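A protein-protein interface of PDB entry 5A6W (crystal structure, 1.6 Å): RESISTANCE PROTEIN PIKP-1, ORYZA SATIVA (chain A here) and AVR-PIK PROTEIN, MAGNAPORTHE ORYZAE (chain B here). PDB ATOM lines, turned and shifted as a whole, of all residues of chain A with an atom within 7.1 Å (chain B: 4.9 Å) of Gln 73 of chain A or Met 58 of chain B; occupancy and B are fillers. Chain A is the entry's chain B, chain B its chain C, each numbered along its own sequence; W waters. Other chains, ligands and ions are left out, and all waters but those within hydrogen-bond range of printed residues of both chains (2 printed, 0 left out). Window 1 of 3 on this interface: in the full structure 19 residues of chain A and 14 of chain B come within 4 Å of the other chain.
Of the 12 printed residues of chain B, 5 touch a printed residue of chain A.
Among the printed residues, 12 pairs touch across the chains.
Among the printed residues, Asp or Glu carboxylates within 4 Å of a Lys or Arg side-chain nitrogen of the other chain: Glu 70 of chain A with Lys 59 of chain B (3.3 Å).
O of Lys 7 of chain A lies within hydrogen-bond range of N of Ser 75 of chain A, at 3.0 Å.
O of Val 9 of chain A lies within hydrogen-bond range of N of Leu 72 of chain A, 2.8 Å away.
The backbone carbonyl oxygen (O) of Gln 73 of chain A lies within hydrogen-bond range of the backbone NH (N) of Val 9 of chain A (2.9 Å).
The side-chain amide nitrogen of Gln 73 of chain A is in hydrogen-bond range of the side-chain hydroxyl of Ser 75 of chain A (2.9 Å).
O of Met 56 of chain B sits at hydrogen-bond distance from N of Ile 67 of chain B, at 2.8 Å.
The backbone NH of Val 65 of chain B lies within hydrogen-bond range of the backbone carbonyl oxygen of Met 58 of chain B (2.9 Å).
Leu 71 of chain A touches Trp 64 of chain B.
Met 58 of chain B touches Leu 72 of chain A.
Leu 72 of chain A touches Trp 64 of chain B.
Met 56 of chain B touches Gln 73 of chain A.
Gln 73 of chain A touches Asp 57 of chain B (CA to O, 3.2 Å).
Met 58 of chain B touches Gln 73 of chain A (CE to OE1, 3.7 Å).
CH2 of Trp 64 of chain B touches N of Gln 73 of chain A (3.8 Å).
Val 74 of chain A touches Met 56 of chain B.
Ser 75 of chain A touches Met 56 of chain B.
Of chain B, only Met 56 (3.8 Å), Asp 57 (3.2 Å), Met 58 (3.7 Å) and Trp 64 (3.8 Å) come within 4 Å of Gln 73 of chain A.
Of the printed residues of chain B, Val 74 of chain A touches Met 56 and Asp 57.
Of the printed residues of chain B, Ser 75 of chain A touches Met 56.
Of the printed residues of chain A, Met 56 of chain B touches Gln 73 (3.8 Å), Val 74 (3.7 Å) and Ser 75 (3.5 Å).
Of the printed residues of chain A, Asp 57 of chain B touches Gln 73 (3.2 Å) and Val 74 (2.9 Å).
Met 58 of chain B touches just these residues of chain A: Leu 72 and Gln 73.
Of the printed residues of chain A, Lys 59 of chain B touches Glu 70 and Leu 72.
The nearest residue of chain B that does not touch Gln 73 of chain A is Trp 36 of chain B (4.4 Å).
NZ of Lys 59 of chain B lies within salt-bridge range of OE2 of Glu 70 of chain A, 3.3 Å away.
N of Lys 59 of chain B sits at hydrogen-bond distance from O of Leu 72 of chain A (2.9 Å).
O of Val 74 of chain A is in hydrogen-bond range of N of Asp 57 of chain B, at 2.9 Å.
Water W2 lies within hydrogen-bond range of O of Leu 71 of chain A (2.7 Å) and NZ of Lys 59 of chain B (3.3 Å).
Water W1 lies within hydrogen-bond range of the side-chain amide oxygen of Gln 73 of chain A and the indole nitrogen of Trp 36 of chain B.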
ATOM      1  N   LYS A   7     -14.863 -31.775   3.461  1.00  0.00           N
ATOM      2  CA  LYS A   7     -16.166 -31.577   2.795  1.00  0.00           C
ATOM      3  C   LYS A   7     -16.611 -30.146   2.914  1.00  0.00           C
ATOM      4  O   LYS A   7     -16.616 -29.589   4.006  1.00  0.00           O
ATOM      5  CB  LYS A   7     -17.243 -32.514   3.343  1.00  0.00           C
ATOM      6  CG  LYS A   7     -18.608 -32.324   2.661  1.00  0.00           C
ATOM      7  CD  LYS A   7     -19.726 -33.152   3.285  1.00  0.00           C
ATOM      8  CE  LYS A   7     -19.589 -34.587   2.920  1.00  0.00           C
ATOM      9  NZ  LYS A   7     -20.643 -35.451   3.540  1.00  0.00           N
ATOM     10  N   ILE A   8     -16.946 -29.548   1.779  1.00  0.00           N
ATOM     11  CA  ILE A   8     -17.484 -28.198   1.778  1.00  0.00           C
ATOM     12  C   ILE A   8     -18.742 -28.116   0.990  1.00  0.00           C
ATOM     13  O   ILE A   8     -18.937 -28.885   0.039  1.00  0.00           O
ATOM     14  CB  ILE A   8     -16.511 -27.139   1.333  1.00  0.00           C
ATOM     15  CG1 ILE A   8     -16.167 -27.306  -0.087  1.00  0.00           C
ATOM     16  CG2 ILE A   8     -15.244 -27.138   2.169  1.00  0.00           C
ATOM     17  CD1 ILE A   8     -15.527 -26.077  -0.679  1.00  0.00           C
ATOM     18  N   VAL A   9     -19.649 -27.247   1.426  1.00  0.00           N
ATOM     19  CA  VAL A   9     -20.902 -27.075   0.710  1.00  0.00           C
ATOM     20  C   VAL A   9     -21.042 -25.616   0.333  1.00  0.00           C
ATOM     21  O   VAL A   9     -20.866 -24.727   1.191  1.00  0.00           O
ATOM     22  CB  VAL A   9     -22.095 -27.505   1.557  1.00  0.00           C
ATOM     23  CG1 VAL A   9     -23.399 -27.333   0.782  1.00  0.00           C
ATOM     24  CG2 VAL A   9     -21.884 -28.960   2.027  1.00  0.00           C
ATOM     25  N   ILE A  10     -21.326 -25.360  -0.939  1.00  0.00           N
ATOM     26  CA  ILE A  10     -21.454 -24.012  -1.492  1.00  0.00           C
ATOM     27  C   ILE A  10     -22.819 -23.874  -2.182  1.00  0.00           C
ATOM     28  O   ILE A  10     -23.244 -24.743  -2.951  1.00  0.00           O
ATOM     29  CB  ILE A  10     -20.323 -23.728  -2.499  1.00  0.00           C
ATOM     30  CG1 ILE A  10     -18.961 -23.731  -1.787  1.00  0.00           C
ATOM     31  CG2 ILE A  10     -20.568 -22.433  -3.237  1.00  0.00           C
ATOM     32  CD1 ILE A  10     -17.790 -23.831  -2.775  1.00  0.00           C
ATOM     33  N   GLU A  47     -21.913 -29.937  -3.018  1.00  0.00           N
ATOM     34  CA  GLU A  47     -21.073 -30.491  -2.009  1.00  0.00           C
ATOM     35  C   GLU A  47     -19.803 -31.047  -2.679  1.00  0.00           C
ATOM     36  O   GLU A  47     -19.903 -31.817  -3.640  1.00  0.00           O
ATOM     37  CB  GLU A  47     -21.901 -31.534  -1.291  1.00  0.00           C
ATOM     38  CG  GLU A  47     -21.298 -32.108  -0.049  1.00  0.00           C
ATOM     39  CD  GLU A  47     -22.310 -33.011   0.621  1.00  0.00           C
ATOM     40  OE1 GLU A  47     -22.474 -34.163   0.180  1.00  0.00           O
ATOM     41  OE2 GLU A  47     -23.022 -32.546   1.521  1.00  0.00           O
ATOM     42  N   PRO A  55     -11.551 -23.379   0.209  1.00  0.00           N
ATOM     43  CA  PRO A  55     -12.957 -23.047  -0.103  1.00  0.00           C
ATOM     44  C   PRO A  55     -13.175 -21.605  -0.485  1.00  0.00           C
ATOM     45  O   PRO A  55     -14.095 -21.284  -1.270  1.00  0.00           O
ATOM     46  CB  PRO A  55     -13.684 -23.327   1.216  1.00  0.00           C
ATOM     47  CG  PRO A  55     -12.774 -24.252   1.954  1.00  0.00           C
ATOM     48  CD  PRO A  55     -11.390 -23.984   1.541  1.00  0.00           C
ATOM     49  N   GLU A  70     -21.972 -18.768  -2.118  1.00  0.00           N
ATOM     50  CA  GLU A  70     -21.913 -18.587  -0.667  1.00  0.00           C
ATOM     51  C   GLU A  70     -21.462 -19.890  -0.036  1.00  0.00           C
ATOM     52  O   GLU A  70     -22.030 -20.931  -0.335  1.00  0.00           O
ATOM     53  CB  GLU A  70     -23.313 -18.255  -0.169  1.00  0.00           C
ATOM     54  CG  GLU A  70     -23.470 -17.926   1.281  1.00  0.00           C
ATOM     55  CD  GLU A  70     -24.936 -17.650   1.630  1.00  0.00           C
ATOM     56  OE1 GLU A  70     -25.841 -17.920   0.789  1.00  0.00           O
ATOM     57  OE2 GLU A  70     -25.174 -17.199   2.757  1.00  0.00           O
ATOM     58  N   LEU A  71     -20.475 -19.818   0.844  1.00  0.00           N
ATOM     59  CA  LEU A  71     -20.022 -20.983   1.607  1.00  0.00           C
ATOM     60  C   LEU A  71     -20.993 -21.285   2.748  1.00  0.00           C
ATOM     61  O   LEU A  71     -21.329 -20.384   3.558  1.00  0.00           O
ATOM     62  CB  LEU A  71     -18.651 -20.700   2.214  1.00  0.00           C
ATOM     63  CG  LEU A  71     -17.978 -21.838   2.950  1.00  0.00           C
ATOM     64  CD1 LEU A  71     -17.741 -23.067   2.087  1.00  0.00           C
ATOM     65  CD2 LEU A  71     -16.637 -21.334   3.476  1.00  0.00           C
ATOM     66  N   LEU A  72     -21.487 -22.526   2.791  1.00  0.00           N
ATOM     67  CA  LEU A  72     -22.492 -22.892   3.808  1.00  0.00           C
ATOM     68  C   LEU A  72     -22.072 -23.925   4.823  1.00  0.00           C
ATOM     69  O   LEU A  72     -22.685 -24.048   5.879  1.00  0.00           O
ATOM     70  CB  LEU A  72     -23.770 -23.375   3.123  1.00  0.00           C
ATOM     71  CG  LEU A  72     -24.473 -22.390   2.202  1.00  0.00           C
ATOM     72  CD1 LEU A  72     -25.702 -23.121   1.647  1.00  0.00           C
ATOM     73  CD2 LEU A  72     -24.878 -21.147   2.933  1.00  0.00           C
ATOM     74  N   GLN A  73     -21.026 -24.719   4.556  1.00  0.00           N
ATOM     75  CA  GLN A  73     -20.596 -25.747   5.500  1.00  0.00           C
ATOM     76  C   GLN A  73     -19.176 -26.117   5.208  1.00  0.00           C
ATOM     77  O   GLN A  73     -18.799 -26.198   4.025  1.00  0.00           O
ATOM     78  CB  GLN A  73     -21.435 -27.042   5.329  1.00  0.00           C
ATOM     79  CG  GLN A  73     -21.140 -28.081   6.355  1.00  0.00           C
ATOM     80  CD  GLN A  73     -21.825 -29.417   6.120  1.00  0.00           C
ATOM     81  OE1 GLN A  73     -23.013 -29.458   5.769  1.00  0.00           O
ATOM     82  NE2 GLN A  73     -21.137 -30.465   6.440  1.00  0.00           N
ATOM     83  N   VAL A  74     -18.433 -26.357   6.305  1.00  0.00           N
ATOM     84  CA  VAL A  74     -17.093 -26.941   6.251  1.00  0.00           C
ATOM     85  C   VAL A  74     -17.076 -28.022   7.327  1.00  0.00           C
ATOM     86  O   VAL A  74     -17.409 -27.762   8.493  1.00  0.00           O
ATOM     87  CB  VAL A  74     -16.012 -25.862   6.533  1.00  0.00           C
ATOM     88  CG1 VAL A  74     -14.633 -26.536   6.494  1.00  0.00           C
ATOM     89  CG2 VAL A  74     -16.090 -24.716   5.568  1.00  0.00           C
ATOM     90  N   SER A  75     -16.703 -29.251   6.953  1.00  0.00           N
ATOM     91  CA  SER A  75     -16.652 -30.333   7.917  1.00  0.00           C
ATOM     92  C   SER A  75     -15.635 -31.385   7.523  1.00  0.00           C
ATOM     93  O   SER A  75     -15.078 -31.297   6.437  1.00  0.00           O
ATOM     94  CB  SER A  75     -18.018 -30.963   8.080  1.00  0.00           C
ATOM     95  OG  SER A  75     -18.444 -31.505   6.880  1.00  0.00           O
ATOM     96  OXT SER A  75     -15.304 -32.243   8.366  1.00  0.00           O
ATOM     97  N   TRP B  36     -29.412 -34.439   9.259  1.00  0.00           N
ATOM     98  CA  TRP B  36     -29.718 -33.191   9.973  1.00  0.00           C
ATOM     99  C   TRP B  36     -30.816 -32.439   9.241  1.00  0.00           C
ATOM    100  O   TRP B  36     -30.962 -32.600   8.019  1.00  0.00           O
ATOM    101  CB  TRP B  36     -28.484 -32.277  10.167  1.00  0.00           C
ATOM    102  CG  TRP B  36     -27.824 -31.829   8.874  1.00  0.00           C
ATOM    103  CD1 TRP B  36     -26.750 -32.455   8.241  1.00  0.00           C
ATOM    104  CD2 TRP B  36     -28.186 -30.730   8.029  1.00  0.00           C
ATOM    105  NE1 TRP B  36     -26.455 -31.815   7.081  1.00  0.00           N
ATOM    106  CE2 TRP B  36     -27.306 -30.751   6.926  1.00  0.00           C
ATOM    107  CE3 TRP B  36     -29.193 -29.760   8.060  1.00  0.00           C
ATOM    108  CZ2 TRP B  36     -27.403 -29.858   5.901  1.00  0.00           C
ATOM    109  CZ3 TRP B  36     -29.243 -28.841   7.049  1.00  0.00           C
ATOM    110  CH2 TRP B  36     -28.399 -28.907   5.987  1.00  0.00           C
ATOM    111  N   MET B  38     -32.665 -28.426   9.292  1.00  0.00           N
ATOM    112  CA  MET B  38     -32.534 -27.050   9.760  1.00  0.00           C
ATOM    113  C   MET B  38     -33.916 -26.400   9.640  1.00  0.00           C
ATOM    114  O   MET B  38     -34.543 -26.496   8.595  1.00  0.00           O
ATOM    115  CB  MET B  38     -31.517 -26.268   8.910  1.00  0.00           C
ATOM    116  CG  MET B  38     -31.380 -24.840   9.374  1.00  0.00           C
ATOM    117  SD  MET B  38     -30.054 -23.947   8.492  1.00  0.00           S
ATOM    118  CE  MET B  38     -28.730 -25.016   8.393  1.00  0.00           C
ATOM    119  N   MET B  56     -18.941 -29.806  12.809  1.00  0.00           N
ATOM    120  CA  MET B  56     -18.933 -29.130  11.516  1.00  0.00           C
ATOM    121  C   MET B  56     -19.195 -27.664  11.758  1.00  0.00           C
ATOM    122  O   MET B  56     -19.731 -27.322  12.820  1.00  0.00           O
ATOM    123  CB  MET B  56     -20.023 -29.701  10.612  1.00  0.00           C
ATOM    124  CG  MET B  56     -21.442 -29.668  11.143  1.00  0.00           C
ATOM    125  SD  MET B  56     -22.584 -30.531   9.996  1.00  0.00           S
ATOM    126  CE  MET B  56     -23.997 -30.694  11.073  1.00  0.00           C
ATOM    127  N   ASP B  57     -18.795 -26.805  10.839  1.00  0.00           N
ATOM    128  CA  ASP B  57     -19.172 -25.407  10.878  1.00  0.00           C
ATOM    129  C   ASP B  57     -20.270 -25.263   9.799  1.00  0.00           C
ATOM    130  O   ASP B  57     -20.055 -25.693   8.648  1.00  0.00           O
ATOM    131  CB  ASP B  57     -18.000 -24.462  10.575  1.00  0.00           C
ATOM    132  CG  ASP B  57     -16.986 -24.375  11.705  1.00  0.00           C
ATOM    133  OD1 ASP B  57     -17.386 -24.497  12.886  1.00  0.00           O
ATOM    134  OD2 ASP B  57     -15.791 -24.130  11.335  1.00  0.00           O
ATOM    135  N   MET B  58     -21.392 -24.630  10.135  1.00  0.00           N
ATOM    136  CA  MET B  58     -22.546 -24.516   9.229  1.00  0.00           C
ATOM    137  C   MET B  58     -23.106 -23.130   9.348  1.00  0.00           C
ATOM    138  O   MET B  58     -23.224 -22.593  10.449  1.00  0.00           O
ATOM    139  CB  MET B  58     -23.575 -25.581   9.560  1.00  0.00           C
ATOM    140  CG  MET B  58     -24.781 -25.543   8.649  1.00  0.00           C
ATOM    141  SD  MET B  58     -26.035 -26.825   9.011  1.00  0.00           S
ATOM    142  CE  MET B  58     -25.187 -28.284   8.468  1.00  0.00           C
ATOM    143  N   LYS B  59     -23.446 -22.535   8.222  1.00  0.00           N
ATOM    144  CA  LYS B  59     -24.154 -21.254   8.205  1.00  0.00           C
ATOM    145  C   LYS B  59     -25.611 -21.532   8.556  1.00  0.00           C
ATOM    146  O   LYS B  59     -26.307 -22.303   7.853  1.00  0.00           O
ATOM    147  CB  LYS B  59     -24.018 -20.606   6.816  1.00  0.00           C
ATOM    148  CG  LYS B  59     -24.638 -19.229   6.742  1.00  0.00           C
ATOM    149  CD  LYS B  59     -23.760 -18.175   7.365  1.00  0.00           C
ATOM    150  CE  LYS B  59     -24.192 -16.787   6.852  1.00  0.00           C
ATOM    151  NZ  LYS B  59     -23.568 -16.493   5.516  1.00  0.00           N
ATOM    152  N   VAL B  60     -26.077 -20.935   9.656  1.00  0.00           N
ATOM    153  CA  VAL B  60     -27.445 -21.093  10.120  1.00  0.00           C
ATOM    154  C   VAL B  60     -27.991 -19.678  10.185  1.00  0.00           C
ATOM    155  O   VAL B  60     -27.636 -18.900  11.069  1.00  0.00           O
ATOM    156  CB  VAL B  60     -27.521 -21.773  11.497  1.00  0.00           C
ATOM    157  CG1 VAL B  60     -28.969 -21.955  11.935  1.00  0.00           C
ATOM    158  CG2 VAL B  60     -26.791 -23.089  11.507  1.00  0.00           C
ATOM    159  N   ASN B  63     -25.594 -16.545  10.949  1.00  0.00           N
ATOM    160  CA  ASN B  63     -24.380 -16.883  11.690  1.00  0.00           C
ATOM    161  C   ASN B  63     -23.679 -18.142  11.258  1.00  0.00           C
ATOM    162  O   ASN B  63     -24.297 -19.129  10.818  1.00  0.00           O
ATOM    163  CB  ASN B  63     -24.725 -17.059  13.185  1.00  0.00           C
ATOM    164  CG  ASN B  63     -25.129 -15.763  13.867  1.00  0.00           C
ATOM    165  OD1 ASN B  63     -25.109 -14.662  13.286  1.00  0.00           O
ATOM    166  ND2 ASN B  63     -25.442 -15.882  15.156  1.00  0.00           N
ATOM    167  N   TRP B  64     -22.351 -18.162  11.442  1.00  0.00           N
ATOM    168  CA  TRP B  64     -21.590 -19.399  11.395  1.00  0.00           C
ATOM    169  C   TRP B  64     -21.721 -20.049  12.752  1.00  0.00           C
ATOM    170  O   TRP B  64     -21.487 -19.384  13.791  1.00  0.00           O
ATOM    171  CB  TRP B  64     -20.114 -19.127  11.071  1.00  0.00           C
ATOM    172  CG  TRP B  64     -19.901 -19.002   9.675  1.00  0.00           C
ATOM    173  CD1 TRP B  64     -19.715 -17.860   8.982  1.00  0.00           C
ATOM    174  CD2 TRP B  64     -19.842 -20.079   8.712  1.00  0.00           C
ATOM    175  NE1 TRP B  64     -19.583 -18.137   7.646  1.00  0.00           N
ATOM    176  CE2 TRP B  64     -19.684 -19.489   7.453  1.00  0.00           C
ATOM    177  CE3 TRP B  64     -19.963 -21.421   8.790  1.00  0.00           C
ATOM    178  CZ2 TRP B  64     -19.592 -20.244   6.300  1.00  0.00           C
ATOM    179  CZ3 TRP B  64     -19.930 -22.188   7.606  1.00  0.00           C
ATOM    180  CH2 TRP B  64     -19.767 -21.594   6.418  1.00  0.00           C
ATOM    181  N   VAL B  65     -22.114 -21.309  12.769  1.00  0.00           N
ATOM    182  CA  VAL B  65     -22.330 -22.037  14.005  1.00  0.00           C
ATOM    183  C   VAL B  65     -21.526 -23.333  14.024  1.00  0.00           C
ATOM    184  O   VAL B  65     -21.552 -24.134  13.084  1.00  0.00           O
ATOM    185  CB  VAL B  65     -23.801 -22.439  14.179  1.00  0.00           C
ATOM    186  CG1 VAL B  65     -24.031 -23.157  15.513  1.00  0.00           C
ATOM    187  CG2 VAL B  65     -24.686 -21.193  14.066  1.00  0.00           C
ATOM    188  N   ILE B  67     -21.267 -26.869  15.150  1.00  0.00           N
ATOM    189  CA  ILE B  67     -22.280 -27.844  15.576  1.00  0.00           C
ATOM    190  C   ILE B  67     -21.565 -29.142  15.886  1.00  0.00           C
ATOM    191  O   ILE B  67     -20.843 -29.657  15.052  1.00  0.00           O
ATOM    192  CB  ILE B  67     -23.321 -28.079  14.474  1.00  0.00           C
ATOM    193  CG1 ILE B  67     -24.014 -26.759  14.074  1.00  0.00           C
ATOM    194  CG2 ILE B  67     -24.354 -29.103  14.920  1.00  0.00           C
ATOM    195  CD1 ILE B  67     -25.036 -26.887  12.957  1.00  0.00           C
ATOM    196  N   VAL B  85     -30.984 -26.664  14.352  1.00  0.00           N
ATOM    197  CA  VAL B  85     -30.595 -27.806  13.518  1.00  0.00           C
ATOM    198  C   VAL B  85     -30.727 -29.027  14.423  1.00  0.00           C
ATOM    199  O   VAL B  85     -30.165 -29.030  15.526  1.00  0.00           O
ATOM    200  CB  VAL B  85     -29.170 -27.688  12.942  1.00  0.00           C
ATOM    201  CG1 VAL B  85     -28.906 -28.812  11.966  1.00  0.00           C
ATOM    202  CG2 VAL B  85     -28.999 -26.356  12.251  1.00  0.00           C
HETATM  203  O   HOH W   1     -24.551 -31.767   4.844  1.00  0.00           O
HETATM  204  O   HOH W   2     -21.144 -17.742   3.722  1.00  0.00           O
